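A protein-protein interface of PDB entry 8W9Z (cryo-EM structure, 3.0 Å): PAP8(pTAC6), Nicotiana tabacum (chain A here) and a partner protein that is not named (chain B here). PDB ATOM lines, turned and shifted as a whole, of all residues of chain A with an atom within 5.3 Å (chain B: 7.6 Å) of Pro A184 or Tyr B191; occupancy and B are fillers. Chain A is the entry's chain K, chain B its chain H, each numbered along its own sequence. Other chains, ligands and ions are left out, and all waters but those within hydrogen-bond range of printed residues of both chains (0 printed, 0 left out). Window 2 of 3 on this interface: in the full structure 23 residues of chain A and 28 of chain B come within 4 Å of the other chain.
Of chain A, only Ala A183 (3.9 Å), Pro A184 (3.4 Å), Arg A259 (3.4 Å), Ala A260 (3.4 Å), Lys A261 (3.2 Å) and Val A262 (2.9 Å) come within 4 Å of Tyr B191. Printed residues of chain B within 4 Å of Ala A260: Tyr B191. Of the printed residues of chain B, Arg A259 touches Tyr B191 and Val B192. Of the printed residues of chain B, Val A262 touches Tyr B191, Val B192 and Ile B193. Printed residues of chain B within 4 Å of Lys A261: Tyr B191 (3.2 Å). Of the printed residues of chain A, Val B192 touches Glu A245 (3.2 Å), Arg A259 (3.9 Å) and Val A262 (3.6 Å). Leu A182 touches none of the printed residues of chain B. Pro A186 touches none of the printed residues of chain B. The nearest residue of chain B that does not touch Pro A184 is Ser B189 (6.6 Å).
Among the printed residues, pairs that only touch across the chains: Ala A183 with Tyr B191 (3.9 Å), Pro A184 with Tyr B191 (3.4 Å), Glu A245 with Val B192 (3.2 Å), Arg A259 with Tyr B191 (3.4 Å), Arg A259 with Val B192 (3.9 Å), Lys A261 with Tyr B191 (3.2 Å) and Val A262 with Val B192 (3.6 Å).
The backbone carbonyl oxygen (O) of Glu A245 sits at hydrogen-bond distance from the guanidinium group (NH1) of Arg A259, 2.8 Å away.
Hydrophobic or aromatic side chains of chain B that line the printed part of chain A: Tyr B191 and Val B192. Among the printed residues, no Asp or Glu carboxylate lies within 4 Å of a Lys or Arg side-chain nitrogen of the other chain.
The backbone NH (N) of Ile B193 is in hydrogen-bond range of the backbone carbonyl oxygen (O) of Val A262. The backbone carbonyl oxygen (O) of Ala A260 sits close to the backbone carbonyl oxygen (O) of Tyr B191 (3.4 Å). N of Val A262 is in hydrogen-bond range of O of Tyr B191 (2.9 Å).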
ATOM      1  N   LEU A 182     -30.438  -0.827  13.572  1.00  0.00           N
ATOM      2  CA  LEU A 182     -29.000  -0.870  13.805  1.00  0.00           C
ATOM      3  C   LEU A 182     -28.657  -0.881  15.292  1.00  0.00           C
ATOM      4  O   LEU A 182     -27.560  -0.459  15.674  1.00  0.00           O
ATOM      5  CB  LEU A 182     -28.313   0.307  13.112  1.00  0.00           C
ATOM      6  CG  LEU A 182     -28.541   0.431  11.605  1.00  0.00           C
ATOM      7  CD1 LEU A 182     -27.839   1.663  11.056  1.00  0.00           C
ATOM      8  CD2 LEU A 182     -28.070  -0.824  10.887  1.00  0.00           C
ATOM      9  N   ALA A 183     -29.568  -1.356  16.137  1.00  0.00           N
ATOM     10  CA  ALA A 183     -29.339  -1.410  17.574  1.00  0.00           C
ATOM     11  C   ALA A 183     -30.298  -2.423  18.173  1.00  0.00           C
ATOM     12  O   ALA A 183     -31.377  -2.650  17.615  1.00  0.00           O
ATOM     13  CB  ALA A 183     -29.539  -0.032  18.221  1.00  0.00           C
ATOM     14  N   PRO A 184     -29.941  -3.053  19.293  1.00  0.00           N
ATOM     15  CA  PRO A 184     -30.873  -3.987  19.940  1.00  0.00           C
ATOM     16  C   PRO A 184     -32.098  -3.251  20.465  1.00  0.00           C
ATOM     17  O   PRO A 184     -31.982  -2.281  21.219  1.00  0.00           O
ATOM     18  CB  PRO A 184     -30.043  -4.592  21.078  1.00  0.00           C
ATOM     19  CG  PRO A 184     -28.965  -3.588  21.335  1.00  0.00           C
ATOM     20  CD  PRO A 184     -28.651  -2.982  19.999  1.00  0.00           C
ATOM     21  N   MET A 185     -33.283  -3.725  20.059  1.00  0.00           N
ATOM     22  CA  MET A 185     -34.532  -3.066  20.401  1.00  0.00           C
ATOM     23  C   MET A 185     -35.192  -3.741  21.597  1.00  0.00           C
ATOM     24  O   MET A 185     -34.977  -4.932  21.844  1.00  0.00           O
ATOM     25  CB  MET A 185     -35.496  -3.088  19.210  1.00  0.00           C
ATOM     26  CG  MET A 185     -34.898  -2.561  17.919  1.00  0.00           C
ATOM     27  SD  MET A 185     -34.072  -0.969  18.114  1.00  0.00           S
ATOM     28  CE  MET A 185     -35.422   0.053  18.694  1.00  0.00           C
ATOM     29  N   PRO A 186     -35.997  -3.004  22.360  1.00  0.00           N
ATOM     30  CA  PRO A 186     -36.677  -3.612  23.507  1.00  0.00           C
ATOM     31  C   PRO A 186     -37.728  -4.616  23.064  1.00  0.00           C
ATOM     32  O   PRO A 186     -38.485  -4.378  22.121  1.00  0.00           O
ATOM     33  CB  PRO A 186     -37.319  -2.417  24.221  1.00  0.00           C
ATOM     34  CG  PRO A 186     -36.611  -1.220  23.696  1.00  0.00           C
ATOM     35  CD  PRO A 186     -36.222  -1.552  22.295  1.00  0.00           C
ATOM     36  N   GLU A 245     -30.600   7.219  29.864  1.00  0.00           N
ATOM     37  CA  GLU A 245     -29.707   6.172  29.389  1.00  0.00           C
ATOM     38  C   GLU A 245     -30.333   5.301  28.309  1.00  0.00           C
ATOM     39  O   GLU A 245     -29.620   4.507  27.688  1.00  0.00           O
ATOM     40  CB  GLU A 245     -29.256   5.295  30.559  1.00  0.00           C
ATOM     41  CG  GLU A 245     -28.115   5.884  31.372  1.00  0.00           C
ATOM     42  CD  GLU A 245     -27.829   5.093  32.634  1.00  0.00           C
ATOM     43  OE1 GLU A 245     -28.297   5.508  33.714  1.00  0.00           O
ATOM     44  OE2 GLU A 245     -27.145   4.051  32.546  1.00  0.00           O
ATOM     45  N   TYR A 248     -33.999   6.379  22.006  1.00  0.00           N
ATOM     46  CA  TYR A 248     -34.015   5.815  20.662  1.00  0.00           C
ATOM     47  C   TYR A 248     -34.305   6.920  19.658  1.00  0.00           C
ATOM     48  O   TYR A 248     -35.376   7.533  19.697  1.00  0.00           O
ATOM     49  CB  TYR A 248     -35.051   4.696  20.553  1.00  0.00           C
ATOM     50  CG  TYR A 248     -34.756   3.528  21.459  1.00  0.00           C
ATOM     51  CD1 TYR A 248     -33.852   2.545  21.081  1.00  0.00           C
ATOM     52  CD2 TYR A 248     -35.372   3.411  22.696  1.00  0.00           C
ATOM     53  CE1 TYR A 248     -33.572   1.478  21.908  1.00  0.00           C
ATOM     54  CE2 TYR A 248     -35.100   2.346  23.529  1.00  0.00           C
ATOM     55  CZ  TYR A 248     -34.198   1.383  23.131  1.00  0.00           C
ATOM     56  OH  TYR A 248     -33.918   0.320  23.957  1.00  0.00           O
ATOM     57  N   ARG A 259     -29.950   3.477  18.804  1.00  0.00           N
ATOM     58  CA  ARG A 259     -29.877   3.904  20.192  1.00  0.00           C
ATOM     59  C   ARG A 259     -28.929   5.091  20.323  1.00  0.00           C
ATOM     60  O   ARG A 259     -28.113   5.366  19.440  1.00  0.00           O
ATOM     61  CB  ARG A 259     -29.412   2.752  21.088  1.00  0.00           C
ATOM     62  CG  ARG A 259     -29.963   2.797  22.504  1.00  0.00           C
ATOM     63  CD  ARG A 259     -29.507   1.586  23.300  1.00  0.00           C
ATOM     64  NE  ARG A 259     -30.187   1.478  24.588  1.00  0.00           N
ATOM     65  CZ  ARG A 259     -29.778   2.075  25.702  1.00  0.00           C
ATOM     66  NH1 ARG A 259     -28.692   2.833  25.691  1.00  0.00           N
ATOM     67  NH2 ARG A 259     -30.458   1.915  26.828  1.00  0.00           N
ATOM     68  N   ALA A 260     -29.047   5.796  21.444  1.00  0.00           N
ATOM     69  CA  ALA A 260     -28.255   6.991  21.704  1.00  0.00           C
ATOM     70  C   ALA A 260     -27.093   6.635  22.623  1.00  0.00           C
ATOM     71  O   ALA A 260     -27.305   6.155  23.741  1.00  0.00           O
ATOM     72  CB  ALA A 260     -29.116   8.089  22.328  1.00  0.00           C
ATOM     73  N   LYS A 261     -25.869   6.872  22.147  1.00  0.00           N
ATOM     74  CA  LYS A 261     -24.662   6.603  22.928  1.00  0.00           C
ATOM     75  C   LYS A 261     -24.486   7.724  23.948  1.00  0.00           C
ATOM     76  O   LYS A 261     -23.687   8.649  23.780  1.00  0.00           O
ATOM     77  CB  LYS A 261     -23.448   6.472  22.016  1.00  0.00           C
ATOM     78  CG  LYS A 261     -23.562   5.360  20.989  1.00  0.00           C
ATOM     79  CD  LYS A 261     -22.309   5.267  20.134  1.00  0.00           C
ATOM     80  CE  LYS A 261     -22.065   6.558  19.369  1.00  0.00           C
ATOM     81  NZ  LYS A 261     -20.842   6.477  18.524  1.00  0.00           N
ATOM     82  N   VAL A 262     -25.254   7.632  25.033  1.00  0.00           N
ATOM     83  CA  VAL A 262     -25.222   8.667  26.056  1.00  0.00           C
ATOM     84  C   VAL A 262     -23.940   8.553  26.871  1.00  0.00           C
ATOM     85  O   VAL A 262     -23.387   7.462  27.066  1.00  0.00           O
ATOM     86  CB  VAL A 262     -26.466   8.581  26.959  1.00  0.00           C
ATOM     87  CG1 VAL A 262     -27.722   8.857  26.153  1.00  0.00           C
ATOM     88  CG2 VAL A 262     -26.546   7.217  27.627  1.00  0.00           C
ATOM     89  N   SER B 188     -24.009  -2.496  32.339  1.00  0.00           N
ATOM     90  CA  SER B 188     -24.087  -1.299  31.512  1.00  0.00           C
ATOM     91  C   SER B 188     -23.666  -1.626  30.085  1.00  0.00           C
ATOM     92  O   SER B 188     -22.570  -2.151  29.857  1.00  0.00           O
ATOM     93  CB  SER B 188     -23.207  -0.196  32.093  1.00  0.00           C
ATOM     94  OG  SER B 188     -23.270   0.978  31.303  1.00  0.00           O
ATOM     95  N   SER B 189     -24.535  -1.318  29.125  1.00  0.00           N
ATOM     96  CA  SER B 189     -24.252  -1.621  27.733  1.00  0.00           C
ATOM     97  C   SER B 189     -23.209  -0.653  27.175  1.00  0.00           C
ATOM     98  O   SER B 189     -22.784   0.301  27.832  1.00  0.00           O
ATOM     99  CB  SER B 189     -25.532  -1.561  26.902  1.00  0.00           C
ATOM    100  OG  SER B 189     -26.483  -2.505  27.362  1.00  0.00           O
ATOM    101  N   GLU B 190     -22.795  -0.917  25.933  1.00  0.00           N
ATOM    102  CA  GLU B 190     -21.817  -0.053  25.282  1.00  0.00           C
ATOM    103  C   GLU B 190     -22.393   1.331  25.003  1.00  0.00           C
ATOM    104  O   GLU B 190     -21.640   2.308  24.914  1.00  0.00           O
ATOM    105  CB  GLU B 190     -21.328  -0.707  23.988  1.00  0.00           C
ATOM    106  CG  GLU B 190     -20.141  -0.016  23.328  1.00  0.00           C
ATOM    107  CD  GLU B 190     -20.555   1.062  22.345  1.00  0.00           C
ATOM    108  OE1 GLU B 190     -21.755   1.128  22.004  1.00  0.00           O
ATOM    109  OE2 GLU B 190     -19.682   1.844  21.915  1.00  0.00           O
ATOM    110  N   TYR B 191     -23.717   1.436  24.880  1.00  0.00           N
ATOM    111  CA  TYR B 191     -24.350   2.713  24.577  1.00  0.00           C
ATOM    112  C   TYR B 191     -24.389   3.659  25.769  1.00  0.00           C
ATOM    113  O   TYR B 191     -24.836   4.800  25.615  1.00  0.00           O
ATOM    114  CB  TYR B 191     -25.768   2.478  24.055  1.00  0.00           C
ATOM    115  CG  TYR B 191     -25.827   1.584  22.838  1.00  0.00           C
ATOM    116  CD1 TYR B 191     -25.470   2.062  21.584  1.00  0.00           C
ATOM    117  CD2 TYR B 191     -26.241   0.264  22.941  1.00  0.00           C
ATOM    118  CE1 TYR B 191     -25.521   1.250  20.470  1.00  0.00           C
ATOM    119  CE2 TYR B 191     -26.296  -0.555  21.831  1.00  0.00           C
ATOM    120  CZ  TYR B 191     -25.935  -0.057  20.599  1.00  0.00           C
ATOM    121  OH  TYR B 191     -25.989  -0.869  19.490  1.00  0.00           O
ATOM    122  N   VAL B 192     -23.942   3.221  26.943  1.00  0.00           N
ATOM    123  CA  VAL B 192     -23.878   4.061  28.133  1.00  0.00           C
ATOM    124  C   VAL B 192     -22.445   4.056  28.644  1.00  0.00           C
ATOM    125  O   VAL B 192     -21.840   2.988  28.797  1.00  0.00           O
ATOM    126  CB  VAL B 192     -24.852   3.583  29.224  1.00  0.00           C
ATOM    127  CG1 VAL B 192     -24.744   4.470  30.451  1.00  0.00           C
ATOM    128  CG2 VAL B 192     -26.277   3.570  28.696  1.00  0.00           C
ATOM    129  N   ILE B 193     -21.905   5.244  28.908  1.00  0.00           N
ATOM    130  CA  ILE B 193     -20.534   5.408  29.373  1.00  0.00           C
ATOM    131  C   ILE B 193     -20.548   6.264  30.631  1.00  0.00           C
ATOM    132  O   ILE B 193     -21.121   7.359  30.635  1.00  0.00           O
ATOM    133  CB  ILE B 193     -19.636   6.047  28.296  1.00  0.00           C
ATOM    134  CG1 ILE B 193     -19.616   5.184  27.032  1.00  0.00           C
ATOM    135  CG2 ILE B 193     -18.227   6.249  28.827  1.00  0.00           C
ATOM    136  CD1 ILE B 193     -19.035   3.803  27.245  1.00  0.00           C
